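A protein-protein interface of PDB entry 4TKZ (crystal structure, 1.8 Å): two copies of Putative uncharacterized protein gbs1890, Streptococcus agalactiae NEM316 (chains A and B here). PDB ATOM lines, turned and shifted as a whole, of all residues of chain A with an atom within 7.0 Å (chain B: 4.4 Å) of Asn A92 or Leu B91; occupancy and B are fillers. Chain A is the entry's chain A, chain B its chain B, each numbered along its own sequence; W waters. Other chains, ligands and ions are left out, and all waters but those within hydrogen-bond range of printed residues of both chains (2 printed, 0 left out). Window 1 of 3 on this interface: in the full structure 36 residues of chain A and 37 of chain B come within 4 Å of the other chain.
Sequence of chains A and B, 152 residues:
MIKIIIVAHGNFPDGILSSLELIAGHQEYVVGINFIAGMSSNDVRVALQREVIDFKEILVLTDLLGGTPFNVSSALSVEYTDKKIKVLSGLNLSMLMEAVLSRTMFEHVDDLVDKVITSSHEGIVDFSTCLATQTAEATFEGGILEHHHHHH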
ATOM      1  N   PHE A  12     -39.338   2.664  -5.466  1.00  0.00           N
ATOM      2  CA  PHE A  12     -38.099   3.298  -4.980  1.00  0.00           C
ATOM      3  C   PHE A  12     -37.318   3.937  -6.139  1.00  0.00           C
ATOM      4  O   PHE A  12     -36.909   5.084  -6.018  1.00  0.00           O
ATOM      5  CB  PHE A  12     -37.266   2.229  -4.235  1.00  0.00           C
ATOM      6  CG  PHE A  12     -35.976   2.716  -3.557  1.00  0.00           C
ATOM      7  CD1 PHE A  12     -35.014   3.470  -4.226  1.00  0.00           C
ATOM      8  CD2 PHE A  12     -35.689   2.288  -2.269  1.00  0.00           C
ATOM      9  CE1 PHE A  12     -33.835   3.848  -3.598  1.00  0.00           C
ATOM     10  CE2 PHE A  12     -34.514   2.665  -1.624  1.00  0.00           C
ATOM     11  CZ  PHE A  12     -33.585   3.444  -2.293  1.00  0.00           C
ATOM     12  N   ILE A  16     -36.564   7.954  -5.986  1.00  0.00           N
ATOM     13  CA  ILE A  16     -35.234   8.562  -5.867  1.00  0.00           C
ATOM     14  C   ILE A  16     -34.875   9.343  -7.138  1.00  0.00           C
ATOM     15  O   ILE A  16     -34.173  10.358  -7.076  1.00  0.00           O
ATOM     16  CB  ILE A  16     -34.132   7.543  -5.470  1.00  0.00           C
ATOM     17  CG1 ILE A  16     -32.902   8.279  -4.924  1.00  0.00           C
ATOM     18  CG2 ILE A  16     -33.747   6.642  -6.640  1.00  0.00           C
ATOM     19  CD1 ILE A  16     -31.910   7.361  -4.252  1.00  0.00           C
ATOM     20  N   LEU A  61     -27.078   0.784  -9.550  1.00  0.00           N
ATOM     21  CA  LEU A  61     -27.278   1.109  -8.149  1.00  0.00           C
ATOM     22  C   LEU A  61     -28.503   0.373  -7.626  1.00  0.00           C
ATOM     23  O   LEU A  61     -29.611   0.577  -8.110  1.00  0.00           O
ATOM     24  CB  LEU A  61     -27.446   2.625  -7.992  1.00  0.00           C
ATOM     25  CG  LEU A  61     -26.322   3.393  -8.693  1.00  0.00           C
ATOM     26  CD1 LEU A  61     -26.545   4.902  -8.534  1.00  0.00           C
ATOM     27  CD2 LEU A  61     -24.970   2.975  -8.107  1.00  0.00           C
ATOM     28  N   THR A  62     -28.312  -0.488  -6.635  1.00  0.00           N
ATOM     29  CA  THR A  62     -29.430  -1.284  -6.142  1.00  0.00           C
ATOM     30  C   THR A  62     -29.668  -1.056  -4.685  1.00  0.00           C
ATOM     31  O   THR A  62     -28.761  -0.640  -3.968  1.00  0.00           O
ATOM     32  CB  THR A  62     -29.193  -2.790  -6.332  1.00  0.00           C
ATOM     33  OG1 THR A  62     -28.160  -3.232  -5.435  1.00  0.00           O
ATOM     34  CG2 THR A  62     -28.798  -3.081  -7.773  1.00  0.00           C
ATOM     35  N   ASP A  63     -30.876  -1.367  -4.230  1.00  0.00           N
ATOM     36  CA  ASP A  63     -31.260  -0.962  -2.887  1.00  0.00           C
ATOM     37  C   ASP A  63     -30.592  -1.742  -1.772  1.00  0.00           C
ATOM     38  O   ASP A  63     -30.050  -1.154  -0.836  1.00  0.00           O
ATOM     39  CB  ASP A  63     -32.787  -0.935  -2.708  1.00  0.00           C
ATOM     40  CG  ASP A  63     -33.472  -2.223  -3.119  1.00  0.00           C
ATOM     41  OD1 ASP A  63     -32.824  -3.135  -3.675  1.00  0.00           O
ATOM     42  OD2 ASP A  63     -34.695  -2.318  -2.879  1.00  0.00           O
ATOM     43  N   SER A  89     -24.831  -2.137  -3.799  1.00  0.00           N
ATOM     44  CA  SER A  89     -26.005  -2.110  -2.927  1.00  0.00           C
ATOM     45  C   SER A  89     -25.890  -0.887  -2.011  1.00  0.00           C
ATOM     46  O   SER A  89     -24.859  -0.210  -2.012  1.00  0.00           O
ATOM     47  CB  SER A  89     -26.097  -3.372  -2.085  1.00  0.00           C
ATOM     48  OG  SER A  89     -24.971  -3.502  -1.239  1.00  0.00           O
ATOM     49  N   GLY A  90     -26.945  -0.611  -1.242  1.00  0.00           N
ATOM     50  CA  GLY A  90     -26.920   0.449  -0.237  1.00  0.00           C
ATOM     51  C   GLY A  90     -27.314   1.813  -0.763  1.00  0.00           C
ATOM     52  O   GLY A  90     -26.982   2.831  -0.162  1.00  0.00           O
ATOM     53  N   LEU A  91     -28.028   1.827  -1.888  1.00  0.00           N
ATOM     54  CA  LEU A  91     -28.345   3.062  -2.607  1.00  0.00           C
ATOM     55  C   LEU A  91     -28.954   4.133  -1.713  1.00  0.00           C
ATOM     56  O   LEU A  91     -29.987   3.903  -1.082  1.00  0.00           O
ATOM     57  CB  LEU A  91     -29.307   2.768  -3.766  1.00  0.00           C
ATOM     58  CG  LEU A  91     -29.954   3.978  -4.447  1.00  0.00           C
ATOM     59  CD1 LEU A  91     -28.893   4.876  -5.078  1.00  0.00           C
ATOM     60  CD2 LEU A  91     -30.953   3.522  -5.496  1.00  0.00           C
ATOM     61  N   ASN A  92     -28.283   5.278  -1.643  1.00  0.00           N
ATOM     62  CA  ASN A  92     -28.842   6.487  -1.002  1.00  0.00           C
ATOM     63  C   ASN A  92     -28.736   7.670  -1.959  1.00  0.00           C
ATOM     64  O   ASN A  92     -28.194   7.523  -3.049  1.00  0.00           O
ATOM     65  CB  ASN A  92     -28.239   6.768   0.387  1.00  0.00           C
ATOM     66  CG  ASN A  92     -26.728   6.909   0.374  1.00  0.00           C
ATOM     67  OD1 ASN A  92     -26.131   7.254  -0.640  1.00  0.00           O
ATOM     68  ND2 ASN A  92     -26.103   6.673   1.536  1.00  0.00           N
ATOM     69  N   LEU A  93     -29.256   8.845  -1.604  1.00  0.00           N
ATOM     70  CA  LEU A  93     -29.213   9.930  -2.579  1.00  0.00           C
ATOM     71  C   LEU A  93     -27.775  10.393  -2.815  1.00  0.00           C
ATOM     72  O   LEU A  93     -27.442  10.855  -3.903  1.00  0.00           O
ATOM     73  CB  LEU A  93     -30.150  11.093  -2.198  1.00  0.00           C
ATOM     74  CG  LEU A  93     -30.345  12.243  -3.201  1.00  0.00           C
ATOM     75  CD1 LEU A  93     -30.781  11.760  -4.560  1.00  0.00           C
ATOM     76  CD2 LEU A  93     -31.366  13.268  -2.671  1.00  0.00           C
ATOM     77  N   SER A  94     -26.921  10.251  -1.804  1.00  0.00           N
ATOM     78  CA  SER A  94     -25.506  10.591  -1.944  1.00  0.00           C
ATOM     79  C   SER A  94     -24.851   9.761  -3.047  1.00  0.00           C
ATOM     80  O   SER A  94     -24.083  10.289  -3.860  1.00  0.00           O
ATOM     81  CB  SER A  94     -24.760  10.332  -0.631  1.00  0.00           C
ATOM     82  OG  SER A  94     -25.094  11.290   0.357  1.00  0.00           O
ATOM     83  N   MET A  95     -25.146   8.469  -3.044  1.00  0.00           N
ATOM     84  CA  MET A  95     -24.611   7.541  -4.045  1.00  0.00           C
ATOM     85  C   MET A  95     -25.023   8.011  -5.438  1.00  0.00           C
ATOM     86  O   MET A  95     -24.195   8.108  -6.352  1.00  0.00           O
ATOM     87  CB  MET A  95     -25.128   6.125  -3.773  1.00  0.00           C
ATOM     88  CG  MET A  95     -24.492   5.065  -4.631  1.00  0.00           C
ATOM     89  SD  MET A  95     -25.124   3.437  -4.223  1.00  0.00           S
ATOM     90  CE  MET A  95     -24.248   3.106  -2.697  1.00  0.00           C
ATOM     91  N   LEU A  96     -26.303   8.342  -5.586  1.00  0.00           N
ATOM     92  CA  LEU A  96     -26.843   8.759  -6.880  1.00  0.00           C
ATOM     93  C   LEU A  96     -26.288  10.099  -7.342  1.00  0.00           C
ATOM     94  O   LEU A  96     -25.888  10.257  -8.499  1.00  0.00           O
ATOM     95  CB  LEU A  96     -28.374   8.831  -6.825  1.00  0.00           C
ATOM     96  CG  LEU A  96     -29.074   9.210  -8.129  1.00  0.00           C
ATOM     97  CD1 LEU A  96     -28.615   8.332  -9.315  1.00  0.00           C
ATOM     98  CD2 LEU A  96     -30.581   9.101  -7.933  1.00  0.00           C
ATOM     99  N   MET A  97     -26.267  11.075  -6.443  1.00  0.00           N
ATOM    100  CA  MET A  97     -25.783  12.393  -6.827  1.00  0.00           C
ATOM    101  C   MET A  97     -24.308  12.333  -7.232  1.00  0.00           C
ATOM    102  O   MET A  97     -23.898  12.959  -8.209  1.00  0.00           O
ATOM    103  CB  MET A  97     -26.010  13.405  -5.700  1.00  0.00           C
ATOM    104  CG  MET A  97     -27.487  13.723  -5.405  1.00  0.00           C
ATOM    105  SD  MET A  97     -28.470  14.224  -6.841  1.00  0.00           S
ATOM    106  CE  MET A  97     -27.526  15.651  -7.389  1.00  0.00           C
ATOM    107  N   VAL A 116     -17.879   7.099  -5.553  1.00  0.00           N
ATOM    108  CA  VAL A 116     -19.305   6.938  -5.294  1.00  0.00           C
ATOM    109  C   VAL A 116     -19.528   6.254  -3.947  1.00  0.00           C
ATOM    110  O   VAL A 116     -20.387   6.659  -3.166  1.00  0.00           O
ATOM    111  CB  VAL A 116     -19.980   6.148  -6.440  1.00  0.00           C
ATOM    112  CG1 VAL A 116     -21.363   5.691  -6.040  1.00  0.00           C
ATOM    113  CG2 VAL A 116     -20.043   7.007  -7.708  1.00  0.00           C
ATOM    114  N   SER A 119     -18.598   8.677  -1.038  1.00  0.00           N
ATOM    115  CA  SER A 119     -19.645   9.668  -0.803  1.00  0.00           C
ATOM    116  C   SER A 119     -20.873   9.039  -0.148  1.00  0.00           C
ATOM    117  O   SER A 119     -21.519   9.669   0.688  1.00  0.00           O
ATOM    118  CB  SER A 119     -20.027  10.378  -2.106  1.00  0.00           C
ATOM    119  OG  SER A 119     -19.011  11.279  -2.517  1.00  0.00           O
ATOM    120  N   SER A 120     -21.186   7.799  -0.530  1.00  0.00           N
ATOM    121  CA  SER A 120     -22.335   7.085   0.019  1.00  0.00           C
ATOM    122  C   SER A 120     -22.199   6.946   1.527  1.00  0.00           C
ATOM    123  O   SER A 120     -23.147   7.191   2.286  1.00  0.00           O
ATOM    124  CB  SER A 120     -22.482   5.698  -0.638  1.00  0.00           C
ATOM    125  OG  SER A 120     -22.539   5.814  -2.041  1.00  0.00           O
ATOM    126  N   HIS A 121     -21.000   6.579   1.959  1.00  0.00           N
ATOM    127  CA  HIS A 121     -20.694   6.419   3.369  1.00  0.00           C
ATOM    128  C   HIS A 121     -20.649   7.770   4.080  1.00  0.00           C
ATOM    129  O   HIS A 121     -21.176   7.919   5.182  1.00  0.00           O
ATOM    130  CB  HIS A 121     -19.341   5.727   3.526  1.00  0.00           C
ATOM    131  CG  HIS A 121     -19.389   4.249   3.309  1.00  0.00           C
ATOM    132  ND1 HIS A 121     -20.021   3.395   4.184  1.00  0.00           N
ATOM    133  CD2 HIS A 121     -18.869   3.469   2.331  1.00  0.00           C
ATOM    134  CE1 HIS A 121     -19.895   2.151   3.751  1.00  0.00           C
ATOM    135  NE2 HIS A 121     -19.207   2.171   2.623  1.00  0.00           N
ATOM    136  N   GLU A 122     -20.010   8.748   3.448  1.00  0.00           N
ATOM    137  CA  GLU A 122     -19.864  10.063   4.053  1.00  0.00           C
ATOM    138  C   GLU A 122     -21.207  10.761   4.219  1.00  0.00           C
ATOM    139  O   GLU A 122     -21.337  11.691   5.017  1.00  0.00           O
ATOM    140  CB  GLU A 122     -18.899  10.926   3.227  1.00  0.00           C
ATOM    141  CG  GLU A 122     -17.461  10.430   3.270  1.00  0.00           C
ATOM    142  CD  GLU A 122     -16.523  11.255   2.420  1.00  0.00           C
ATOM    143  OE1 GLU A 122     -16.944  11.712   1.339  1.00  0.00           O
ATOM    144  OE2 GLU A 122     -15.359  11.440   2.835  1.00  0.00           O
ATOM    145  N   GLY A 123     -22.207  10.315   3.466  1.00  0.00           N
ATOM    146  CA  GLY A 123     -23.527  10.927   3.512  1.00  0.00           C
ATOM    147  C   GLY A 123     -24.397  10.461   4.671  1.00  0.00           C
ATOM    148  O   GLY A 123     -25.459  11.030   4.929  1.00  0.00           O
ATOM    149  N   ILE A 124     -23.957   9.410   5.354  1.00  0.00           N
ATOM    150  CA  ILE A 124     -24.678   8.870   6.508  1.00  0.00           C
ATOM    151  C   ILE A 124     -24.177   9.569   7.758  1.00  0.00           C
ATOM    152  O   ILE A 124     -23.068   9.314   8.224  1.00  0.00           O
ATOM    153  CB  ILE A 124     -24.449   7.352   6.645  1.00  0.00           C
ATOM    154  CG1 ILE A 124     -24.977   6.634   5.404  1.00  0.00           C
ATOM    155  CG2 ILE A 124     -25.160   6.804   7.883  1.00  0.00           C
ATOM    156  CD1 ILE A 124     -24.541   5.163   5.310  1.00  0.00           C
ATOM    157  N   ILE B   6     -39.883   9.718   7.619  1.00  0.00           N
ATOM    158  CA  ILE B   6     -38.985   9.867   6.487  1.00  0.00           C
ATOM    159  C   ILE B   6     -39.249  11.196   5.801  1.00  0.00           C
ATOM    160  O   ILE B   6     -40.376  11.441   5.353  1.00  0.00           O
ATOM    161  CB  ILE B   6     -39.243   8.755   5.457  1.00  0.00           C
ATOM    162  CG1 ILE B   6     -39.003   7.371   6.073  1.00  0.00           C
ATOM    163  CG2 ILE B   6     -38.332   8.923   4.244  1.00  0.00           C
ATOM    164  CD1 ILE B   6     -39.377   6.217   5.145  1.00  0.00           C
ATOM    165  N   PHE B  12     -39.396  10.487  -3.112  1.00  0.00           N
ATOM    166  CA  PHE B  12     -38.480   9.509  -2.503  1.00  0.00           C
ATOM    167  C   PHE B  12     -39.115   8.870  -1.247  1.00  0.00           C
ATOM    168  O   PHE B  12     -39.038   7.655  -1.081  1.00  0.00           O
ATOM    169  CB  PHE B  12     -37.151  10.241  -2.221  1.00  0.00           C
ATOM    170  CG  PHE B  12     -36.048   9.423  -1.558  1.00  0.00           C
ATOM    171  CD1 PHE B  12     -36.277   8.621  -0.449  1.00  0.00           C
ATOM    172  CD2 PHE B  12     -34.741   9.568  -2.005  1.00  0.00           C
ATOM    173  CE1 PHE B  12     -35.245   7.926   0.153  1.00  0.00           C
ATOM    174  CE2 PHE B  12     -33.695   8.887  -1.402  1.00  0.00           C
ATOM    175  CZ  PHE B  12     -33.952   8.060  -0.322  1.00  0.00           C
ATOM    176  N   ILE B  16     -39.470   4.798  -1.174  1.00  0.00           N
ATOM    177  CA  ILE B  16     -38.779   3.887  -0.262  1.00  0.00           C
ATOM    178  C   ILE B  16     -39.787   3.213   0.664  1.00  0.00           C
ATOM    179  O   ILE B  16     -39.610   2.058   1.050  1.00  0.00           O
ATOM    180  CB  ILE B  16     -37.641   4.589   0.539  1.00  0.00           C
ATOM    181  CG1 ILE B  16     -36.772   3.548   1.249  1.00  0.00           C
ATOM    182  CG2 ILE B  16     -38.201   5.605   1.542  1.00  0.00           C
ATOM    183  CD1 ILE B  16     -35.473   4.116   1.783  1.00  0.00           C
ATOM    184  N   LEU B  61     -35.499   9.967   9.427  1.00  0.00           N
ATOM    185  CA  LEU B  61     -34.571   9.547   8.392  1.00  0.00           C
ATOM    186  C   LEU B  61     -34.701  10.481   7.192  1.00  0.00           C
ATOM    187  O   LEU B  61     -35.780  10.603   6.609  1.00  0.00           O
ATOM    188  CB  LEU B  61     -34.856   8.090   7.975  1.00  0.00           C
ATOM    189  CG  LEU B  61     -34.902   7.083   9.127  1.00  0.00           C
ATOM    190  CD1 LEU B  61     -35.166   5.678   8.602  1.00  0.00           C
ATOM    191  CD2 LEU B  61     -33.591   7.107   9.912  1.00  0.00           C
ATOM    192  N   THR B  62     -33.601  11.131   6.816  1.00  0.00           N
ATOM    193  CA  THR B  62     -33.620  12.102   5.727  1.00  0.00           C
ATOM    194  C   THR B  62     -32.628  11.750   4.638  1.00  0.00           C
ATOM    195  O   THR B  62     -31.689  10.988   4.872  1.00  0.00           O
ATOM    196  CB  THR B  62     -33.334  13.540   6.245  1.00  0.00           C
ATOM    197  OG1 THR B  62     -31.964  13.639   6.664  1.00  0.00           O
ATOM    198  CG2 THR B  62     -34.232  13.850   7.409  1.00  0.00           C
ATOM    199  N   ASP B  63     -32.826  12.296   3.443  1.00  0.00           N
ATOM    200  CA  ASP B  63     -32.034  11.838   2.305  1.00  0.00           C
ATOM    201  C   ASP B  63     -30.587  12.301   2.292  1.00  0.00           C
ATOM    202  O   ASP B  63     -29.666  11.500   2.106  1.00  0.00           O
ATOM    203  CB  ASP B  63     -32.717  12.128   0.954  1.00  0.00           C
ATOM    204  CG  ASP B  63     -33.146  13.572   0.791  1.00  0.00           C
ATOM    205  OD1 ASP B  63     -32.982  14.372   1.731  1.00  0.00           O
ATOM    206  OD2 ASP B  63     -33.664  13.904  -0.299  1.00  0.00           O
ATOM    207  N   SER B  89     -28.984  11.602   8.150  1.00  0.00           N
ATOM    208  CA  SER B  89     -28.944  11.751   6.702  1.00  0.00           C
ATOM    209  C   SER B  89     -28.406  10.446   6.129  1.00  0.00           C
ATOM    210  O   SER B  89     -27.940   9.585   6.886  1.00  0.00           O
ATOM    211  CB  SER B  89     -28.038  12.897   6.288  1.00  0.00           C
ATOM    212  OG  SER B  89     -26.729  12.690   6.774  1.00  0.00           O
ATOM    213  N   GLY B  90     -28.479  10.297   4.806  1.00  0.00           N
ATOM    214  CA  GLY B  90     -27.915   9.131   4.128  1.00  0.00           C
ATOM    215  C   GLY B  90     -28.850   7.955   3.949  1.00  0.00           C
ATOM    216  O   GLY B  90     -28.400   6.823   3.741  1.00  0.00           O
ATOM    217  N   LEU B  91     -30.150   8.221   4.021  1.00  0.00           N
ATOM    218  CA  LEU B  91     -31.172   7.183   4.026  1.00  0.00           C
ATOM    219  C   LEU B  91     -31.035   6.181   2.877  1.00  0.00           C
ATOM    220  O   LEU B  91     -31.109   6.557   1.707  1.00  0.00           O
ATOM    221  CB  LEU B  91     -32.561   7.824   3.957  1.00  0.00           C
ATOM    222  CG  LEU B  91     -33.758   6.893   3.735  1.00  0.00           C
ATOM    223  CD1 LEU B  91     -33.933   5.963   4.913  1.00  0.00           C
ATOM    224  CD2 LEU B  91     -35.017   7.715   3.535  1.00  0.00           C
ATOM    225  N   ASN B  92     -30.827   4.918   3.229  1.00  0.00           N
ATOM    226  CA  ASN B  92     -30.923   3.810   2.264  1.00  0.00           C
ATOM    227  C   ASN B  92     -31.914   2.781   2.799  1.00  0.00           C
ATOM    228  O   ASN B  92     -32.426   2.944   3.909  1.00  0.00           O
ATOM    229  CB  ASN B  92     -29.551   3.198   1.931  1.00  0.00           C
ATOM    230  CG  ASN B  92     -28.758   2.788   3.159  1.00  0.00           C
ATOM    231  OD1 ASN B  92     -29.314   2.498   4.222  1.00  0.00           O
ATOM    232  ND2 ASN B  92     -27.435   2.749   3.007  1.00  0.00           N
ATOM    233  N   MET B  95     -31.013   1.324   6.199  1.00  0.00           N
ATOM    234  CA  MET B  95     -31.311   2.228   7.317  1.00  0.00           C
ATOM    235  C   MET B  95     -32.762   2.040   7.743  1.00  0.00           C
ATOM    236  O   MET B  95     -33.054   1.850   8.930  1.00  0.00           O
ATOM    237  CB  MET B  95     -31.056   3.678   6.911  1.00  0.00           C
ATOM    238  CG  MET B  95     -31.132   4.653   8.070  1.00  0.00           C
ATOM    239  SD  MET B  95     -30.825   6.330   7.520  1.00  0.00           S
ATOM    240  CE  MET B  95     -29.046   6.300   7.324  1.00  0.00           C
ATOM    241  N   LEU B  96     -33.668   2.063   6.768  1.00  0.00           N
ATOM    242  CA  LEU B  96     -35.098   1.930   7.043  1.00  0.00           C
ATOM    243  C   LEU B  96     -35.486   0.560   7.604  1.00  0.00           C
ATOM    244  O   LEU B  96     -36.229   0.478   8.590  1.00  0.00           O
ATOM    245  CB  LEU B  96     -35.916   2.245   5.778  1.00  0.00           C
ATOM    246  CG  LEU B  96     -37.435   2.127   5.927  1.00  0.00           C
ATOM    247  CD1 LEU B  96     -37.902   2.948   7.118  1.00  0.00           C
ATOM    248  CD2 LEU B  96     -38.124   2.595   4.659  1.00  0.00           C
HETATM  249  O   HOH W   1     -27.551  10.329   1.068  1.00  0.00           O
HETATM  250  O   HOH W   2     -30.685   9.164   0.779  1.00  0.00           O
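The backbone carbonyl oxygen of Gly A90 lies within hydrogen-bond range of the side-chain amide nitrogen of Asn B92.
The backbone carbonyl oxygen of Gly B90 sits at hydrogen-bond distance from the side-chain amide nitrogen of Asn A92, 3.2 Å away.
The backbone carbonyl oxygen of Gly A123 lies within hydrogen-bond range of the side-chain hydroxyl of Ser B89 (2.8 Å).
The backbone NH of Gly B90 is in hydrogen-bond range of the backbone carbonyl oxygen of Gly A123, at 3.1 Å.
The backbone carbonyl oxygen of Thr A62 sits at hydrogen-bond distance from the backbone NH of Gly A90 (3.3 Å).
The backbone carbonyl oxygen (O) of Asp A63 sits at hydrogen-bond distance from the backbone NH (N) of Gly A90 (3.2 Å).
The side-chain amide oxygen of Asn A92 lies close to the backbone NH of Ser A94, at 3.3 Å.
The backbone carbonyl oxygen of Ser A120 is in hydrogen-bond range of the side-chain amide nitrogen of Asn A92, at 3.1 Å.
The backbone carbonyl oxygen of Thr B62 lies within hydrogen-bond range of the backbone NH of Gly B90, at 3.3 Å.
The backbone NH of Leu B91 lies within hydrogen-bond range of the backbone carbonyl oxygen of Thr B62.
Phe A12 touches Ile B16 (CE2 to CG1, 3.8 Å).
Ile A16 touches Phe B12 (CG1 to CE2, 3.7 Å).
Asn B92 touches Leu A91.
Leu B91 touches Asn A92.
Asp B63 touches Leu A93.
Ile A124 touches Ser B89 (CA to O, 3.4 Å).
Ile A124 touches Gly B90.
Met B95 touches Ile A124 (CE to CG2, 3.96 Å).
Asn A92 touches just these residues of chain B: Gly B90 (3.2 Å) and Leu B91 (3.2 Å).
Of the printed residues of chain B, Gly A90 touches Asn B92.
Printed residues of chain B within 4 Å of Gly A123: Ser B89 and Gly B90.
Of the printed residues of chain B, Phe A12 touches Ile B16 (3.8 Å).
Thr A62 touches none of the printed residues of chain B.
The nearest residue of chain B that does not touch Asn A92 is Asn B92 (4.1 Å).
The nearest printed residue of chain A that does not touch Leu B91 is Leu A91 (4.01 Å).
Printed residues of chain A that touch a printed residue of chain B: Phe A12, Ile A16, Gly A90, Leu A91, Asn A92, Leu A93, Gly A123 and Ile A124.
Among the printed residues, no Asp or Glu carboxylate lies within 4 Å of a Lys or Arg side-chain nitrogen of the other chain.
Phe A12 touches Ile B16, and with the chains exchanged Ile A16 touches Phe B12.
Gly A90 touches Asn B92, and with the chains exchanged Asn A92 touches Gly B90.
Leu A91 touches Asn B92, and with the chains exchanged Asn A92 touches Leu B91.
Of the 12 pairs that touch across the chains among the printed residues, 6 have their exchanged pair printed and touching as well.
Water W1 lies within hydrogen-bond range of the backbone carbonyl oxygen of Asp B63 (2.6 Å), the side-chain hydroxyl of Ser A94 (2.7 Å) and the backbone NH of Leu A93 (3.5 Å).
Water W2 lies within hydrogen-bond range of the backbone NH (N) of Leu A93, the backbone carbonyl oxygen (O) of Leu B91 and the backbone carbonyl oxygen (O) of Asp B63.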
